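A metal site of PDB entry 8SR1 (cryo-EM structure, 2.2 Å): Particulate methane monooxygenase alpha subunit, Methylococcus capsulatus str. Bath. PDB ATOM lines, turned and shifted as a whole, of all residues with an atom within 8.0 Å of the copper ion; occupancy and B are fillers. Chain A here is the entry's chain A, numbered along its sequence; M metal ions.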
ATOM      1  N   MET A  12      27.993 -27.685  16.613  1.00  0.00           N
ATOM      2  CA  MET A  12      27.498 -26.338  16.832  1.00  0.00           C
ATOM      3  C   MET A  12      27.126 -26.103  18.296  1.00  0.00           C
ATOM      4  O   MET A  12      27.445 -25.042  18.852  1.00  0.00           O
ATOM      5  CB  MET A  12      26.284 -26.066  15.944  1.00  0.00           C
ATOM      6  CG  MET A  12      26.629 -25.764  14.497  1.00  0.00           C
ATOM      7  SD  MET A  12      25.226 -26.037  13.396  1.00  0.00           S
ATOM      8  CE  MET A  12      25.825 -25.258  11.909  1.00  0.00           C
ATOM      9  N   ARG A  13      26.453 -27.057  18.931  1.00  0.00           N
ATOM     10  CA  ARG A  13      26.012 -26.867  20.305  1.00  0.00           C
ATOM     11  C   ARG A  13      26.675 -27.900  21.215  1.00  0.00           C
ATOM     12  O   ARG A  13      26.034 -28.838  21.684  1.00  0.00           O
ATOM     13  CB  ARG A  13      24.484 -27.004  20.350  1.00  0.00           C
ATOM     14  CG  ARG A  13      23.776 -26.612  19.070  1.00  0.00           C
ATOM     15  CD  ARG A  13      22.488 -27.403  18.864  1.00  0.00           C
ATOM     16  NE  ARG A  13      21.595 -27.347  20.014  1.00  0.00           N
ATOM     17  CZ  ARG A  13      20.756 -26.345  20.259  1.00  0.00           C
ATOM     18  NH1 ARG A  13      20.673 -25.296  19.470  1.00  0.00           N
ATOM     19  NH2 ARG A  13      19.985 -26.413  21.337  1.00  0.00           N
ATOM     20  N   THR A  14      27.971 -27.711  21.470  1.00  0.00           N
ATOM     21  CA  THR A  14      28.582 -28.282  22.658  1.00  0.00           C
ATOM     22  C   THR A  14      29.401 -27.241  23.400  1.00  0.00           C
ATOM     23  O   THR A  14      29.120 -26.908  24.557  1.00  0.00           O
ATOM     24  CB  THR A  14      29.459 -29.482  22.294  1.00  0.00           C
ATOM     25  OG1 THR A  14      30.111 -29.240  21.040  1.00  0.00           O
ATOM     26  CG2 THR A  14      28.626 -30.749  22.192  1.00  0.00           C
ATOM     27  N   ILE A  15      30.397 -26.684  22.713  1.00  0.00           N
ATOM     28  CA  ILE A  15      31.410 -25.818  23.300  1.00  0.00           C
ATOM     29  C   ILE A  15      31.872 -24.851  22.217  1.00  0.00           C
ATOM     30  O   ILE A  15      32.247 -25.273  21.115  1.00  0.00           O
ATOM     31  CB  ILE A  15      32.605 -26.623  23.846  1.00  0.00           C
ATOM     32  CG1 ILE A  15      32.256 -27.251  25.192  1.00  0.00           C
ATOM     33  CG2 ILE A  15      33.831 -25.735  23.972  1.00  0.00           C
ATOM     34  CD1 ILE A  15      33.316 -28.197  25.700  1.00  0.00           C
ATOM     35  N   HIS A  16      31.848 -23.557  22.529  1.00  0.00           N
ATOM     36  CA  HIS A  16      32.242 -22.527  21.573  1.00  0.00           C
ATOM     37  C   HIS A  16      33.605 -21.978  21.975  1.00  0.00           C
ATOM     38  O   HIS A  16      33.766 -21.411  23.065  1.00  0.00           O
ATOM     39  CB  HIS A  16      31.199 -21.411  21.526  1.00  0.00           C
ATOM     40  CG  HIS A  16      29.822 -21.899  21.218  1.00  0.00           C
ATOM     41  ND1 HIS A  16      28.694 -21.384  21.836  1.00  0.00           N
ATOM     42  CD2 HIS A  16      29.380 -22.853  20.369  1.00  0.00           C
ATOM     43  CE1 HIS A  16      27.633 -22.000  21.368  1.00  0.00           C
ATOM     44  NE2 HIS A  16      28.014 -22.895  20.476  1.00  0.00           N
ATOM     45  N   TRP A  17      34.593 -22.159  21.100  1.00  0.00           N
ATOM     46  CA  TRP A  17      35.951 -21.687  21.330  1.00  0.00           C
ATOM     47  C   TRP A  17      36.119 -20.318  20.673  1.00  0.00           C
ATOM     48  O   TRP A  17      35.792 -20.149  19.501  1.00  0.00           O
ATOM     49  CB  TRP A  17      36.976 -22.664  20.754  1.00  0.00           C
ATOM     50  CG  TRP A  17      36.747 -24.098  21.121  1.00  0.00           C
ATOM     51  CD1 TRP A  17      35.855 -24.958  20.531  1.00  0.00           C
ATOM     52  CD2 TRP A  17      37.423 -24.845  22.135  1.00  0.00           C
ATOM     53  NE1 TRP A  17      35.935 -26.194  21.135  1.00  0.00           N
ATOM     54  CE2 TRP A  17      36.882 -26.148  22.117  1.00  0.00           C
ATOM     55  CE3 TRP A  17      38.415 -24.541  23.064  1.00  0.00           C
ATOM     56  CZ2 TRP A  17      37.318 -27.150  22.983  1.00  0.00           C
ATOM     57  CZ3 TRP A  17      38.842 -25.531  23.922  1.00  0.00           C
ATOM     58  CH2 TRP A  17      38.293 -26.820  23.884  1.00  0.00           C
ATOM     59  N   TYR A  18      36.633 -19.353  21.431  1.00  0.00           N
ATOM     60  CA  TYR A  18      36.897 -18.036  20.890  1.00  0.00           C
ATOM     61  C   TYR A  18      38.047 -17.399  21.674  1.00  0.00           C
ATOM     62  O   TYR A  18      38.488 -17.922  22.694  1.00  0.00           O
ATOM     63  CB  TYR A  18      35.643 -17.150  20.931  1.00  0.00           C
ATOM     64  CG  TYR A  18      35.150 -16.790  22.312  1.00  0.00           C
ATOM     65  CD1 TYR A  18      34.401 -17.686  23.053  1.00  0.00           C
ATOM     66  CD2 TYR A  18      35.408 -15.545  22.858  1.00  0.00           C
ATOM     67  CE1 TYR A  18      33.944 -17.362  24.319  1.00  0.00           C
ATOM     68  CE2 TYR A  18      34.962 -15.209  24.117  1.00  0.00           C
ATOM     69  CZ  TYR A  18      34.225 -16.122  24.846  1.00  0.00           C
ATOM     70  OH  TYR A  18      33.771 -15.794  26.092  1.00  0.00           O
ATOM     71  N   PHE A  39      36.653 -20.954  26.156  1.00  0.00           N
ATOM     72  CA  PHE A  39      35.586 -21.812  25.667  1.00  0.00           C
ATOM     73  C   PHE A  39      34.356 -21.619  26.543  1.00  0.00           C
ATOM     74  O   PHE A  39      34.461 -21.470  27.764  1.00  0.00           O
ATOM     75  CB  PHE A  39      35.998 -23.300  25.623  1.00  0.00           C
ATOM     76  CG  PHE A  39      36.326 -23.892  26.964  1.00  0.00           C
ATOM     77  CD1 PHE A  39      35.339 -24.497  27.735  1.00  0.00           C
ATOM     78  CD2 PHE A  39      37.623 -23.874  27.450  1.00  0.00           C
ATOM     79  CE1 PHE A  39      35.632 -25.046  28.957  1.00  0.00           C
ATOM     80  CE2 PHE A  39      37.926 -24.433  28.672  1.00  0.00           C
ATOM     81  CZ  PHE A  39      36.931 -25.014  29.426  1.00  0.00           C
ATOM     82  N   HIS A  40      33.191 -21.612  25.905  1.00  0.00           N
ATOM     83  CA  HIS A  40      31.906 -21.442  26.583  1.00  0.00           C
ATOM     84  C   HIS A  40      31.111 -22.727  26.431  1.00  0.00           C
ATOM     85  O   HIS A  40      30.932 -23.229  25.321  1.00  0.00           O
ATOM     86  CB  HIS A  40      31.136 -20.258  26.010  1.00  0.00           C
ATOM     87  CG  HIS A  40      29.740 -20.135  26.550  1.00  0.00           C
ATOM     88  ND1 HIS A  40      28.626 -20.290  25.770  1.00  0.00           N
ATOM     89  CD2 HIS A  40      29.295 -19.879  27.803  1.00  0.00           C
ATOM     90  CE1 HIS A  40      27.546 -20.134  26.504  1.00  0.00           C
ATOM     91  NE2 HIS A  40      27.921 -19.876  27.743  1.00  0.00           N
ATOM     92  N   VAL A  41      30.620 -23.253  27.553  1.00  0.00           N
ATOM     93  CA  VAL A  41      29.795 -24.455  27.538  1.00  0.00           C
ATOM     94  C   VAL A  41      28.371 -24.053  27.217  1.00  0.00           C
ATOM     95  O   VAL A  41      27.748 -23.281  27.967  1.00  0.00           O
ATOM     96  CB  VAL A  41      29.882 -25.200  28.877  1.00  0.00           C
ATOM     97  CG1 VAL A  41      29.211 -26.553  28.778  1.00  0.00           C
ATOM     98  CG2 VAL A  41      31.329 -25.348  29.307  1.00  0.00           C
ATOM     99  N   PHE A  42      27.839 -24.559  26.111  1.00  0.00           N
ATOM    100  CA  PHE A  42      26.539 -24.128  25.626  1.00  0.00           C
ATOM    101  C   PHE A  42      25.435 -24.570  26.580  1.00  0.00           C
ATOM    102  O   PHE A  42      25.453 -25.691  27.108  1.00  0.00           O
ATOM    103  CB  PHE A  42      26.289 -24.675  24.229  1.00  0.00           C
ATOM    104  CG  PHE A  42      24.983 -24.244  23.641  1.00  0.00           C
ATOM    105  CD1 PHE A  42      24.635 -22.907  23.589  1.00  0.00           C
ATOM    106  CD2 PHE A  42      24.092 -25.170  23.119  1.00  0.00           C
ATOM    107  CE1 PHE A  42      23.434 -22.501  23.040  1.00  0.00           C
ATOM    108  CE2 PHE A  42      22.892 -24.773  22.568  1.00  0.00           C
ATOM    109  CZ  PHE A  42      22.562 -23.440  22.539  1.00  0.00           C
ATOM    110  N   GLU A  43      24.458 -23.682  26.803  1.00  0.00           N
ATOM    111  CA  GLU A  43      23.349 -24.002  27.711  1.00  0.00           C
ATOM    112  C   GLU A  43      22.494 -25.148  27.168  1.00  0.00           C
ATOM    113  O   GLU A  43      22.056 -26.015  27.925  1.00  0.00           O
ATOM    114  CB  GLU A  43      22.490 -22.763  27.941  1.00  0.00           C
ATOM    115  CG  GLU A  43      23.123 -21.735  28.862  1.00  0.00           C
ATOM    116  CD  GLU A  43      24.070 -20.806  28.144  1.00  0.00           C
ATOM    117  OE1 GLU A  43      24.277 -20.986  26.928  1.00  0.00           O
ATOM    118  OE2 GLU A  43      24.611 -19.876  28.785  1.00  0.00           O
ATOM    119  N   GLY A  44      22.247 -25.162  25.864  1.00  0.00           N
ATOM    120  CA  GLY A  44      21.470 -26.220  25.257  1.00  0.00           C
ATOM    121  C   GLY A  44      22.297 -27.459  24.971  1.00  0.00           C
ATOM    122  O   GLY A  44      22.333 -27.949  23.841  1.00  0.00           O
ATOM    123  N   GLY A  87      26.838 -23.497  30.676  1.00  0.00           N
ATOM    124  CA  GLY A  87      26.571 -22.075  30.622  1.00  0.00           C
ATOM    125  C   GLY A  87      27.714 -21.195  31.065  1.00  0.00           C
ATOM    126  O   GLY A  87      27.634 -19.971  30.911  1.00  0.00           O
ATOM    127  N   LYS A  88      28.787 -21.778  31.600  1.00  0.00           N
ATOM    128  CA  LYS A  88      29.927 -21.017  32.079  1.00  0.00           C
ATOM    129  C   LYS A  88      30.981 -20.886  30.990  1.00  0.00           C
ATOM    130  O   LYS A  88      31.118 -21.730  30.107  1.00  0.00           O
ATOM    131  CB  LYS A  88      30.531 -21.671  33.320  1.00  0.00           C
ATOM    132  CG  LYS A  88      29.638 -21.600  34.545  1.00  0.00           C
ATOM    133  CD  LYS A  88      29.571 -20.183  35.094  1.00  0.00           C
ATOM    134  CE  LYS A  88      28.333 -19.987  35.950  1.00  0.00           C
ATOM    135  NZ  LYS A  88      28.404 -18.754  36.767  1.00  0.00           N
ATOM    136  N   THR A  89      31.739 -19.791  31.066  1.00  0.00           N
ATOM    137  CA  THR A  89      32.856 -19.545  30.174  1.00  0.00           C
ATOM    138  C   THR A  89      34.154 -19.690  30.956  1.00  0.00           C
ATOM    139  O   THR A  89      34.296 -19.111  32.036  1.00  0.00           O
ATOM    140  CB  THR A  89      32.779 -18.149  29.542  1.00  0.00           C
ATOM    141  OG1 THR A  89      31.541 -18.008  28.840  1.00  0.00           O
ATOM    142  CG2 THR A  89      33.935 -17.930  28.589  1.00  0.00           C
ATOM    143  N   TYR A 286      30.279 -16.811  14.842  1.00  0.00           N
ATOM    144  CA  TYR A 286      30.991 -18.071  15.031  1.00  0.00           C
ATOM    145  C   TYR A 286      29.963 -19.148  15.315  1.00  0.00           C
ATOM    146  O   TYR A 286      29.169 -19.013  16.247  1.00  0.00           O
ATOM    147  CB  TYR A 286      32.005 -17.933  16.175  1.00  0.00           C
ATOM    148  CG  TYR A 286      32.569 -19.231  16.718  1.00  0.00           C
ATOM    149  CD1 TYR A 286      31.872 -19.983  17.661  1.00  0.00           C
ATOM    150  CD2 TYR A 286      33.818 -19.674  16.317  1.00  0.00           C
ATOM    151  CE1 TYR A 286      32.390 -21.161  18.161  1.00  0.00           C
ATOM    152  CE2 TYR A 286      34.345 -20.852  16.818  1.00  0.00           C
ATOM    153  CZ  TYR A 286      33.631 -21.581  17.743  1.00  0.00           C
ATOM    154  OH  TYR A 286      34.158 -22.759  18.244  1.00  0.00           O
ATOM    155  N   THR A 287      29.978 -20.220  14.522  1.00  0.00           N
ATOM    156  CA  THR A 287      28.979 -21.288  14.667  1.00  0.00           C
ATOM    157  C   THR A 287      29.613 -22.589  15.136  1.00  0.00           C
ATOM    158  O   THR A 287      29.232 -23.107  16.192  1.00  0.00           O
ATOM    159  CB  THR A 287      28.209 -21.485  13.358  1.00  0.00           C
ATOM    160  OG1 THR A 287      27.454 -22.691  13.424  1.00  0.00           O
ATOM    161  CG2 THR A 287      29.151 -21.516  12.147  1.00  0.00           C
ATOM    162  N   ALA A 356      23.599 -23.429  17.041  1.00  0.00           N
ATOM    163  CA  ALA A 356      23.968 -22.461  18.058  1.00  0.00           C
ATOM    164  C   ALA A 356      25.262 -21.781  17.623  1.00  0.00           C
ATOM    165  O   ALA A 356      26.039 -22.338  16.846  1.00  0.00           O
ATOM    166  CB  ALA A 356      24.149 -23.108  19.440  1.00  0.00           C
ATOM    167  N   GLY A 357      25.474 -20.583  18.142  1.00  0.00           N
ATOM    168  CA  GLY A 357      26.669 -19.849  17.767  1.00  0.00           C
ATOM    169  C   GLY A 357      26.871 -18.636  18.659  1.00  0.00           C
ATOM    170  O   GLY A 357      26.142 -18.424  19.627  1.00  0.00           O
ATOM    171  N   LEU A 358      27.890 -17.862  18.310  1.00  0.00           N
ATOM    172  CA  LEU A 358      28.227 -16.639  19.027  1.00  0.00           C
ATOM    173  C   LEU A 358      28.238 -15.476  18.048  1.00  0.00           C
ATOM    174  O   LEU A 358      28.829 -15.579  16.971  1.00  0.00           O
ATOM    175  CB  LEU A 358      29.577 -16.754  19.719  1.00  0.00           C
ATOM    176  CG  LEU A 358      29.755 -17.836  20.782  1.00  0.00           C
ATOM    177  CD1 LEU A 358      31.174 -17.795  21.331  1.00  0.00           C
ATOM    178  CD2 LEU A 358      28.745 -17.675  21.897  1.00  0.00           C
ATOM    179  N   VAL A 370      29.825 -10.180  23.352  1.00  0.00           N
ATOM    180  CA  VAL A 370      29.574 -11.538  22.907  1.00  0.00           C
ATOM    181  C   VAL A 370      28.159 -11.911  23.319  1.00  0.00           C
ATOM    182  O   VAL A 370      27.816 -11.883  24.506  1.00  0.00           O
ATOM    183  CB  VAL A 370      30.582 -12.534  23.501  1.00  0.00           C
ATOM    184  CG1 VAL A 370      30.385 -13.915  22.883  1.00  0.00           C
ATOM    185  CG2 VAL A 370      32.001 -12.047  23.278  1.00  0.00           C
ATOM    186  N   VAL A 371      27.328 -12.267  22.328  1.00  0.00           N
ATOM    187  CA  VAL A 371      25.984 -12.749  22.593  1.00  0.00           C
ATOM    188  C   VAL A 371      25.835 -14.097  21.916  1.00  0.00           C
ATOM    189  O   VAL A 371      26.404 -14.368  20.863  1.00  0.00           O
ATOM    190  CB  VAL A 371      24.890 -11.760  22.110  1.00  0.00           C
ATOM    191  CG1 VAL A 371      25.249 -10.336  22.501  1.00  0.00           C
ATOM    192  CG2 VAL A 371      24.680 -11.857  20.618  1.00  0.00           C
ATOM    193  N   GLN A 372      25.068 -14.974  22.566  1.00  0.00           N
ATOM    194  CA  GLN A 372      24.871 -16.336  22.096  1.00  0.00           C
ATOM    195  C   GLN A 372      23.480 -16.477  21.499  1.00  0.00           C
ATOM    196  O   GLN A 372      22.500 -15.988  22.069  1.00  0.00           O
ATOM    197  CB  GLN A 372      25.068 -17.332  23.241  1.00  0.00           C
ATOM    198  CG  GLN A 372      24.799 -18.765  22.860  1.00  0.00           C
ATOM    199  CD  GLN A 372      25.356 -19.731  23.874  1.00  0.00           C
ATOM    200  OE1 GLN A 372      26.418 -20.325  23.674  1.00  0.00           O
ATOM    201  NE2 GLN A 372      24.643 -19.904  24.979  1.00  0.00           N
ATOM    202  N   ILE A 373      23.389 -17.143  20.355  1.00  0.00           N
ATOM    203  CA  ILE A 373      22.133 -17.361  19.657  1.00  0.00           C
ATOM    204  C   ILE A 373      21.972 -18.841  19.373  1.00  0.00           C
ATOM    205  O   ILE A 373      22.953 -19.547  19.107  1.00  0.00           O
ATOM    206  CB  ILE A 373      22.051 -16.541  18.346  1.00  0.00           C
ATOM    207  CG1 ILE A 373      23.254 -16.834  17.455  1.00  0.00           C
ATOM    208  CG2 ILE A 373      21.946 -15.056  18.657  1.00  0.00           C
ATOM    209  CD1 ILE A 373      23.089 -16.372  16.036  1.00  0.00           C
HETATM  210 CU    CU M   1      28.634 -21.202  23.908  1.00  0.00          CU
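Phe 42 touches the copper ion (CA to CU, 3.99 Å).
Of the 25 residues printed, 4 come within 4 Å of the copper ion.
The nearest printed residue that does not touch the copper ion is Leu 358 (4.1 Å).
The backbone NH (N) of Phe 42 lies within hydrogen-bond range of the backbone carbonyl oxygen (O) of Thr 14, 3.1 Å away.
The side-chain carboxylate (OE2) of Glu 43 lies within hydrogen-bond range of a ring nitrogen (NE2) of His 40, at 3.5 Å.
O of Met 12 lies within hydrogen-bond range of NE2 of His 16, at 2.8 Å.
A ring nitrogen (NE2) of His 40 sits at hydrogen-bond distance from the backbone carbonyl oxygen (O) of Gly 87 (3.2 Å).
The copper ion is bound by a ring nitrogen (ND1) of His 40 (2.1 Å), a ring nitrogen (ND1) of His 16 (2.1 Å) and the side-chain amide oxygen (OE1) of Gln 372 (2.4 Å).
The copper ion has three donor atoms within binding distance.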
